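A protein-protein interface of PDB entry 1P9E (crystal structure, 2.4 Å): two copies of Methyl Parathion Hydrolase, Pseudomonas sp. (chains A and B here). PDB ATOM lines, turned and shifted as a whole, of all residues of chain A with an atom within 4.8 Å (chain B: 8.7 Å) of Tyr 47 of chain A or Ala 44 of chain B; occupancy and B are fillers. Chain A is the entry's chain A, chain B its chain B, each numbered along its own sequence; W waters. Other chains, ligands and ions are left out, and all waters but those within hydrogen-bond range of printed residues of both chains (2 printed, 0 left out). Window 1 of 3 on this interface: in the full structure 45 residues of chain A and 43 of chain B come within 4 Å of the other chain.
The guanidinium group of Arg 49 of chain A is in hydrogen-bond range of the backbone carbonyl oxygen of Thr 42 of chain B (2.7 Å).
Water W2 bridges the side-chain hydroxyl (OG) of Ser 43 of chain B (2.6 Å) and the backbone carbonyl oxygen (O) of Arg 49 of chain A (2.9 Å).
Water W1 lies within hydrogen-bond range of the backbone NH (N) of Ala 44 of chain B (2.8 Å) and the backbone NH (N) of Arg 49 of chain A (3.0 Å).
NH2 of Arg 49 of chain A lies within hydrogen-bond range of O of Ala 133 of chain A, 2.6 Å away.
NH1 of Arg 49 of chain A sits at hydrogen-bond distance from OG1 of Thr 58 of chain A, 2.8 Å away.
Pro 45 of chain A touches Tyr 47 of chain B.
O of Ser 43 of chain B touches OH of Tyr 47 of chain A, 3.95 Å away.
Tyr 47 of chain A touches Ala 44 of chain B.
OH of Tyr 47 of chain A touches CD of Pro 45 of chain B (3.8 Å).
Val 40 of chain B touches Arg 49 of chain A (CG1 to NH2, 3.7 Å).
Phe 305 of chain A touches Tyr 325 of chain B (CB to CG, 3.7 Å).
Of the printed residues of chain B, Tyr 47 of chain A touches Ser 43, Ala 44 and Pro 45.
Of the printed residues of chain A, Thr 42 of chain B touches Arg 49.
Of the printed residues of chain A, Tyr 47 of chain B touches Pro 45.
The nearest residue of chain B that does not touch Tyr 47 of chain A is Thr 42 of chain B (4.3 Å).
Pro 45 of chain A touches Tyr 47 of chain B, and with the chains exchanged Tyr 47 of chain A touches Pro 45 of chain B.
Positions printed for both chains: 45, 46, 47, 129, 132 and 305.
Of the 7 pairs that touch across the chains among the printed residues, 2 have their exchanged pair printed and touching as well.
Of the 12 printed residues of chain A, 4 touch a printed residue of chain B.
Printed residues of chain A that touch a printed residue of chain B: Pro 45, Tyr 47, Arg 49 and Phe 305.
Hydrophobic or aromatic side chains of chain A within 4 Å of the printed part of chain B: Pro 45, Tyr 47 and Phe 305.
Along chain A the printed residues that touch a printed residue of chain B span positions 45 to 305.
Of the 14 printed residues of chain B, 7 touch a printed residue of chain A.
Printed residues of chain B that touch a printed residue of chain A: Val 40, Thr 42, Ser 43, Ala 44, Pro 45, Tyr 47 and Tyr 325.
Hydrophobic or aromatic side chains of chain B within 4 Å of the printed part of chain A: Val 40, Ala 44, Pro 45, Tyr 47 and Tyr 325.
Along chain B the printed residues that touch a printed residue of chain A span positions 40 to 325.
Among the printed residues, 7 pairs touch across the chains.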
ATOM      1  N   PRO A  45     -10.051 -19.983   0.687  1.00  0.00           N
ATOM      2  CA  PRO A  45      -9.214 -20.223   1.882  1.00  0.00           C
ATOM      3  C   PRO A  45      -8.530 -21.578   1.670  1.00  0.00           C
ATOM      4  O   PRO A  45      -9.168 -22.535   1.233  1.00  0.00           O
ATOM      5  CB  PRO A  45     -10.235 -20.283   3.025  1.00  0.00           C
ATOM      6  CG  PRO A  45     -11.363 -19.372   2.538  1.00  0.00           C
ATOM      7  CD  PRO A  45     -11.464 -19.743   1.058  1.00  0.00           C
ATOM      8  N   GLY A  46      -7.248 -21.674   1.986  1.00  0.00           N
ATOM      9  CA  GLY A  46      -6.542 -22.913   1.731  1.00  0.00           C
ATOM     10  C   GLY A  46      -6.689 -24.062   2.707  1.00  0.00           C
ATOM     11  O   GLY A  46      -5.695 -24.525   3.268  1.00  0.00           O
ATOM     12  N   TYR A  47      -7.905 -24.539   2.928  1.00  0.00           N
ATOM     13  CA  TYR A  47      -8.057 -25.667   3.837  1.00  0.00           C
ATOM     14  C   TYR A  47      -9.122 -26.594   3.262  1.00  0.00           C
ATOM     15  O   TYR A  47     -10.042 -26.141   2.574  1.00  0.00           O
ATOM     16  CB  TYR A  47      -8.408 -25.183   5.257  1.00  0.00           C
ATOM     17  CG  TYR A  47      -9.797 -24.599   5.454  1.00  0.00           C
ATOM     18  CD1 TYR A  47     -10.836 -25.372   5.993  1.00  0.00           C
ATOM     19  CD2 TYR A  47     -10.064 -23.266   5.149  1.00  0.00           C
ATOM     20  CE1 TYR A  47     -12.109 -24.821   6.230  1.00  0.00           C
ATOM     21  CE2 TYR A  47     -11.330 -22.700   5.378  1.00  0.00           C
ATOM     22  CZ  TYR A  47     -12.342 -23.481   5.919  1.00  0.00           C
ATOM     23  OH  TYR A  47     -13.576 -22.923   6.163  1.00  0.00           O
ATOM     24  N   TYR A  48      -8.969 -27.893   3.513  1.00  0.00           N
ATOM     25  CA  TYR A  48      -9.912 -28.875   3.000  1.00  0.00           C
ATOM     26  C   TYR A  48     -10.297 -29.828   4.148  1.00  0.00           C
ATOM     27  O   TYR A  48      -9.416 -30.461   4.752  1.00  0.00           O
ATOM     28  CB  TYR A  48      -9.233 -29.630   1.855  1.00  0.00           C
ATOM     29  CG  TYR A  48     -10.087 -30.645   1.143  1.00  0.00           C
ATOM     30  CD1 TYR A  48     -10.659 -30.345  -0.089  1.00  0.00           C
ATOM     31  CD2 TYR A  48     -10.319 -31.907   1.699  1.00  0.00           C
ATOM     32  CE1 TYR A  48     -11.443 -31.273  -0.760  1.00  0.00           C
ATOM     33  CE2 TYR A  48     -11.101 -32.844   1.040  1.00  0.00           C
ATOM     34  CZ  TYR A  48     -11.662 -32.524  -0.190  1.00  0.00           C
ATOM     35  OH  TYR A  48     -12.442 -33.438  -0.874  1.00  0.00           O
ATOM     36  N   ARG A  49     -11.599 -29.930   4.434  1.00  0.00           N
ATOM     37  CA  ARG A  49     -12.118 -30.772   5.516  1.00  0.00           C
ATOM     38  C   ARG A  49     -12.470 -32.200   5.090  1.00  0.00           C
ATOM     39  O   ARG A  49     -13.074 -32.423   4.040  1.00  0.00           O
ATOM     40  CB  ARG A  49     -13.377 -30.132   6.136  1.00  0.00           C
ATOM     41  CG  ARG A  49     -13.649 -30.564   7.594  1.00  0.00           C
ATOM     42  CD  ARG A  49     -12.766 -29.782   8.562  1.00  0.00           C
ATOM     43  NE  ARG A  49     -13.159 -28.374   8.644  1.00  0.00           N
ATOM     44  CZ  ARG A  49     -12.521 -27.466   9.371  1.00  0.00           C
ATOM     45  NH1 ARG A  49     -11.451 -27.815  10.078  1.00  0.00           N
ATOM     46  NH2 ARG A  49     -12.952 -26.209   9.397  1.00  0.00           N
ATOM     47  N   THR A  58      -7.936 -31.859   8.316  1.00  0.00           N
ATOM     48  CA  THR A  58      -8.075 -30.621   7.580  1.00  0.00           C
ATOM     49  C   THR A  58      -6.728 -30.412   6.913  1.00  0.00           C
ATOM     50  O   THR A  58      -5.728 -30.240   7.598  1.00  0.00           O
ATOM     51  CB  THR A  58      -8.347 -29.398   8.479  1.00  0.00           C
ATOM     52  OG1 THR A  58      -9.462 -29.655   9.348  1.00  0.00           O
ATOM     53  CG2 THR A  58      -8.659 -28.172   7.600  1.00  0.00           C
ATOM     54  N   ALA A  59      -6.681 -30.494   5.590  1.00  0.00           N
ATOM     55  CA  ALA A  59      -5.426 -30.239   4.890  1.00  0.00           C
ATOM     56  C   ALA A  59      -5.356 -28.706   4.876  1.00  0.00           C
ATOM     57  O   ALA A  59      -6.378 -28.020   4.635  1.00  0.00           O
ATOM     58  CB  ALA A  59      -5.477 -30.794   3.444  1.00  0.00           C
ATOM     59  N   LEU A  60      -4.162 -28.186   5.145  1.00  0.00           N
ATOM     60  CA  LEU A  60      -3.889 -26.766   5.212  1.00  0.00           C
ATOM     61  C   LEU A  60      -2.823 -26.490   4.176  1.00  0.00           C
ATOM     62  O   LEU A  60      -1.739 -27.077   4.230  1.00  0.00           O
ATOM     63  CB  LEU A  60      -3.332 -26.413   6.590  1.00  0.00           C
ATOM     64  CG  LEU A  60      -4.245 -26.722   7.775  1.00  0.00           C
ATOM     65  CD1 LEU A  60      -3.488 -26.531   9.106  1.00  0.00           C
ATOM     66  CD2 LEU A  60      -5.459 -25.809   7.688  1.00  0.00           C
ATOM     67  N   ASN A 129      -4.411 -20.176   7.048  1.00  0.00           N
ATOM     68  CA  ASN A 129      -5.383 -21.205   6.709  1.00  0.00           C
ATOM     69  C   ASN A 129      -5.811 -21.994   7.944  1.00  0.00           C
ATOM     70  O   ASN A 129      -6.964 -22.425   8.047  1.00  0.00           O
ATOM     71  CB  ASN A 129      -4.820 -22.129   5.619  1.00  0.00           C
ATOM     72  CG  ASN A 129      -4.839 -21.467   4.257  1.00  0.00           C
ATOM     73  OD1 ASN A 129      -5.804 -20.777   3.923  1.00  0.00           O
ATOM     74  ND2 ASN A 129      -3.789 -21.676   3.460  1.00  0.00           N
ATOM     75  N   ALA A 132      -8.412 -19.726   9.478  1.00  0.00           N
ATOM     76  CA  ALA A 132      -9.626 -19.739   8.644  1.00  0.00           C
ATOM     77  C   ALA A 132     -10.305 -21.112   8.780  1.00  0.00           C
ATOM     78  O   ALA A 132     -11.530 -21.235   8.646  1.00  0.00           O
ATOM     79  CB  ALA A 132      -9.281 -19.461   7.185  1.00  0.00           C
ATOM     80  N   ALA A 133      -9.497 -22.136   9.046  1.00  0.00           N
ATOM     81  CA  ALA A 133     -10.002 -23.497   9.231  1.00  0.00           C
ATOM     82  C   ALA A 133     -10.798 -23.600  10.530  1.00  0.00           C
ATOM     83  O   ALA A 133     -11.386 -24.641  10.816  1.00  0.00           O
ATOM     84  CB  ALA A 133      -8.845 -24.498   9.254  1.00  0.00           C
ATOM     85  N   PHE A 305      -2.938 -29.941  -3.969  1.00  0.00           N
ATOM     86  CA  PHE A 305      -3.745 -29.691  -2.768  1.00  0.00           C
ATOM     87  C   PHE A 305      -5.192 -30.093  -3.052  1.00  0.00           C
ATOM     88  O   PHE A 305      -5.706 -29.809  -4.136  1.00  0.00           O
ATOM     89  CB  PHE A 305      -3.678 -28.194  -2.410  1.00  0.00           C
ATOM     90  CG  PHE A 305      -4.525 -27.812  -1.230  1.00  0.00           C
ATOM     91  CD1 PHE A 305      -4.080 -28.060   0.073  1.00  0.00           C
ATOM     92  CD2 PHE A 305      -5.803 -27.259  -1.423  1.00  0.00           C
ATOM     93  CE1 PHE A 305      -4.895 -27.769   1.176  1.00  0.00           C
ATOM     94  CE2 PHE A 305      -6.634 -26.966  -0.335  1.00  0.00           C
ATOM     95  CZ  PHE A 305      -6.182 -27.221   0.970  1.00  0.00           C
ATOM     96  N   VAL B  40     -14.356 -28.816  14.484  1.00  0.00           N
ATOM     97  CA  VAL B  40     -15.177 -27.811  13.825  1.00  0.00           C
ATOM     98  C   VAL B  40     -16.155 -28.511  12.888  1.00  0.00           C
ATOM     99  O   VAL B  40     -17.368 -28.327  12.987  1.00  0.00           O
ATOM    100  CB  VAL B  40     -14.297 -26.804  13.047  1.00  0.00           C
ATOM    101  CG1 VAL B  40     -15.167 -25.788  12.308  1.00  0.00           C
ATOM    102  CG2 VAL B  40     -13.366 -26.082  14.015  1.00  0.00           C
ATOM    103  N   ARG B  41     -15.631 -29.317  11.977  1.00  0.00           N
ATOM    104  CA  ARG B  41     -16.478 -30.059  11.049  1.00  0.00           C
ATOM    105  C   ARG B  41     -17.334 -29.283  10.061  1.00  0.00           C
ATOM    106  O   ARG B  41     -18.532 -29.557   9.926  1.00  0.00           O
ATOM    107  CB  ARG B  41     -17.396 -31.007  11.814  1.00  0.00           C
ATOM    108  CG  ARG B  41     -16.656 -32.067  12.549  1.00  0.00           C
ATOM    109  CD  ARG B  41     -17.565 -33.250  12.826  1.00  0.00           C
ATOM    110  NE  ARG B  41     -16.823 -34.306  13.495  1.00  0.00           N
ATOM    111  CZ  ARG B  41     -17.077 -35.594  13.357  1.00  0.00           C
ATOM    112  NH1 ARG B  41     -18.067 -35.970  12.565  1.00  0.00           N
ATOM    113  NH2 ARG B  41     -16.330 -36.500  13.991  1.00  0.00           N
ATOM    114  N   THR B  42     -16.733 -28.320   9.375  1.00  0.00           N
ATOM    115  CA  THR B  42     -17.445 -27.582   8.344  1.00  0.00           C
ATOM    116  C   THR B  42     -16.503 -27.558   7.157  1.00  0.00           C
ATOM    117  O   THR B  42     -15.283 -27.453   7.335  1.00  0.00           O
ATOM    118  CB  THR B  42     -17.746 -26.154   8.755  1.00  0.00           C
ATOM    119  OG1 THR B  42     -16.528 -25.524   9.169  1.00  0.00           O
ATOM    120  CG2 THR B  42     -18.765 -26.131   9.877  1.00  0.00           C
ATOM    121  N   SER B  43     -17.053 -27.681   5.950  1.00  0.00           N
ATOM    122  CA  SER B  43     -16.214 -27.657   4.759  1.00  0.00           C
ATOM    123  C   SER B  43     -15.863 -26.206   4.457  1.00  0.00           C
ATOM    124  O   SER B  43     -16.511 -25.287   4.971  1.00  0.00           O
ATOM    125  CB  SER B  43     -16.948 -28.296   3.570  1.00  0.00           C
ATOM    126  OG  SER B  43     -17.128 -29.699   3.773  1.00  0.00           O
ATOM    127  N   ALA B  44     -14.847 -25.984   3.628  1.00  0.00           N
ATOM    128  CA  ALA B  44     -14.479 -24.610   3.293  1.00  0.00           C
ATOM    129  C   ALA B  44     -15.534 -24.070   2.361  1.00  0.00           C
ATOM    130  O   ALA B  44     -16.355 -24.834   1.852  1.00  0.00           O
ATOM    131  CB  ALA B  44     -13.160 -24.583   2.610  1.00  0.00           C
ATOM    132  N   PRO B  45     -15.554 -22.742   2.141  1.00  0.00           N
ATOM    133  CA  PRO B  45     -16.571 -22.199   1.225  1.00  0.00           C
ATOM    134  C   PRO B  45     -16.428 -22.965  -0.095  1.00  0.00           C
ATOM    135  O   PRO B  45     -15.317 -23.312  -0.512  1.00  0.00           O
ATOM    136  CB  PRO B  45     -16.173 -20.727   1.112  1.00  0.00           C
ATOM    137  CG  PRO B  45     -15.612 -20.438   2.469  1.00  0.00           C
ATOM    138  CD  PRO B  45     -14.743 -21.658   2.729  1.00  0.00           C
ATOM    139  N   GLY B  46     -17.544 -23.252  -0.739  1.00  0.00           N
ATOM    140  CA  GLY B  46     -17.481 -24.010  -1.969  1.00  0.00           C
ATOM    141  C   GLY B  46     -17.235 -23.193  -3.228  1.00  0.00           C
ATOM    142  O   GLY B  46     -18.120 -23.086  -4.081  1.00  0.00           O
ATOM    143  N   TYR B  47     -16.053 -22.601  -3.359  1.00  0.00           N
ATOM    144  CA  TYR B  47     -15.745 -21.854  -4.580  1.00  0.00           C
ATOM    145  C   TYR B  47     -14.279 -22.072  -4.941  1.00  0.00           C
ATOM    146  O   TYR B  47     -13.394 -22.070  -4.080  1.00  0.00           O
ATOM    147  CB  TYR B  47     -16.098 -20.364  -4.425  1.00  0.00           C
ATOM    148  CG  TYR B  47     -15.177 -19.547  -3.565  1.00  0.00           C
ATOM    149  CD1 TYR B  47     -14.114 -18.841  -4.136  1.00  0.00           C
ATOM    150  CD2 TYR B  47     -15.373 -19.448  -2.187  1.00  0.00           C
ATOM    151  CE1 TYR B  47     -13.270 -18.047  -3.350  1.00  0.00           C
ATOM    152  CE2 TYR B  47     -14.531 -18.661  -1.391  1.00  0.00           C
ATOM    153  CZ  TYR B  47     -13.485 -17.961  -1.985  1.00  0.00           C
ATOM    154  OH  TYR B  47     -12.657 -17.151  -1.240  1.00  0.00           O
ATOM    155  N   SER B  61     -19.861 -24.423  -6.138  1.00  0.00           N
ATOM    156  CA  SER B  61     -20.495 -25.651  -5.688  1.00  0.00           C
ATOM    157  C   SER B  61     -21.897 -25.367  -5.137  1.00  0.00           C
ATOM    158  O   SER B  61     -22.094 -24.439  -4.351  1.00  0.00           O
ATOM    159  CB  SER B  61     -19.647 -26.300  -4.591  1.00  0.00           C
ATOM    160  OG  SER B  61     -20.302 -27.436  -4.075  1.00  0.00           O
ATOM    161  N   ARG B 125     -26.629 -24.303  -2.388  1.00  0.00           N
ATOM    162  CA  ARG B 125     -25.615 -23.446  -1.773  1.00  0.00           C
ATOM    163  C   ARG B 125     -24.901 -22.532  -2.765  1.00  0.00           C
ATOM    164  O   ARG B 125     -24.044 -21.724  -2.362  1.00  0.00           O
ATOM    165  CB  ARG B 125     -24.557 -24.285  -1.053  1.00  0.00           C
ATOM    166  CG  ARG B 125     -25.091 -25.263  -0.015  1.00  0.00           C
ATOM    167  CD  ARG B 125     -23.902 -25.839   0.733  1.00  0.00           C
ATOM    168  NE  ARG B 125     -24.269 -26.838   1.724  1.00  0.00           N
ATOM    169  CZ  ARG B 125     -23.417 -27.319   2.623  1.00  0.00           C
ATOM    170  NH1 ARG B 125     -22.160 -26.872   2.643  1.00  0.00           N
ATOM    171  NH2 ARG B 125     -23.809 -28.259   3.486  1.00  0.00           N
ATOM    172  N   ASN B 129     -22.349 -19.545  -1.900  1.00  0.00           N
ATOM    173  CA  ASN B 129     -20.958 -19.650  -2.365  1.00  0.00           C
ATOM    174  C   ASN B 129     -20.554 -18.499  -3.299  1.00  0.00           C
ATOM    175  O   ASN B 129     -19.388 -18.076  -3.307  1.00  0.00           O
ATOM    176  CB  ASN B 129     -20.709 -21.012  -3.030  1.00  0.00           C
ATOM    177  CG  ASN B 129     -20.477 -22.129  -2.001  1.00  0.00           C
ATOM    178  OD1 ASN B 129     -19.633 -21.997  -1.134  1.00  0.00           O
ATOM    179  ND2 ASN B 129     -21.223 -23.226  -2.105  1.00  0.00           N
ATOM    180  N   ALA B 132     -19.662 -15.863  -1.070  1.00  0.00           N
ATOM    181  CA  ALA B 132     -18.391 -16.203  -0.441  1.00  0.00           C
ATOM    182  C   ALA B 132     -17.277 -15.886  -1.455  1.00  0.00           C
ATOM    183  O   ALA B 132     -16.166 -15.485  -1.082  1.00  0.00           O
ATOM    184  CB  ALA B 132     -18.360 -17.681  -0.087  1.00  0.00           C
ATOM    185  N   PHE B 305     -16.206 -31.751  -7.497  1.00  0.00           N
ATOM    186  CA  PHE B 305     -15.900 -30.324  -7.369  1.00  0.00           C
ATOM    187  C   PHE B 305     -14.387 -30.061  -7.399  1.00  0.00           C
ATOM    188  O   PHE B 305     -13.635 -30.796  -6.766  1.00  0.00           O
ATOM    189  CB  PHE B 305     -16.493 -29.765  -6.062  1.00  0.00           C
ATOM    190  CG  PHE B 305     -16.428 -28.250  -5.967  1.00  0.00           C
ATOM    191  CD1 PHE B 305     -17.220 -27.455  -6.797  1.00  0.00           C
ATOM    192  CD2 PHE B 305     -15.516 -27.626  -5.114  1.00  0.00           C
ATOM    193  CE1 PHE B 305     -17.090 -26.065  -6.781  1.00  0.00           C
ATOM    194  CE2 PHE B 305     -15.381 -26.246  -5.091  1.00  0.00           C
ATOM    195  CZ  PHE B 305     -16.167 -25.459  -5.929  1.00  0.00           C
ATOM    196  N   TYR B 325      -4.009 -27.923  -8.650  1.00  0.00           N
ATOM    197  CA  TYR B 325      -4.288 -26.823  -7.736  1.00  0.00           C
ATOM    198  C   TYR B 325      -3.436 -25.618  -8.079  1.00  0.00           C
ATOM    199  O   TYR B 325      -2.223 -25.735  -8.234  1.00  0.00           O
ATOM    200  CB  TYR B 325      -3.982 -27.192  -6.293  1.00  0.00           C
ATOM    201  CG  TYR B 325      -4.272 -26.057  -5.346  1.00  0.00           C
ATOM    202  CD1 TYR B 325      -5.586 -25.680  -5.066  1.00  0.00           C
ATOM    203  CD2 TYR B 325      -3.236 -25.361  -4.722  1.00  0.00           C
ATOM    204  CE1 TYR B 325      -5.871 -24.641  -4.182  1.00  0.00           C
ATOM    205  CE2 TYR B 325      -3.495 -24.316  -3.833  1.00  0.00           C
ATOM    206  CZ  TYR B 325      -4.821 -23.954  -3.560  1.00  0.00           C
ATOM    207  OH  TYR B 325      -5.094 -22.924  -2.670  1.00  0.00           O
HETATM  208  O   HOH W   1     -13.536 -28.299   2.783  1.00  0.00           O
HETATM  209  O   HOH W   2     -15.014 -30.825   2.653  1.00  0.00           O
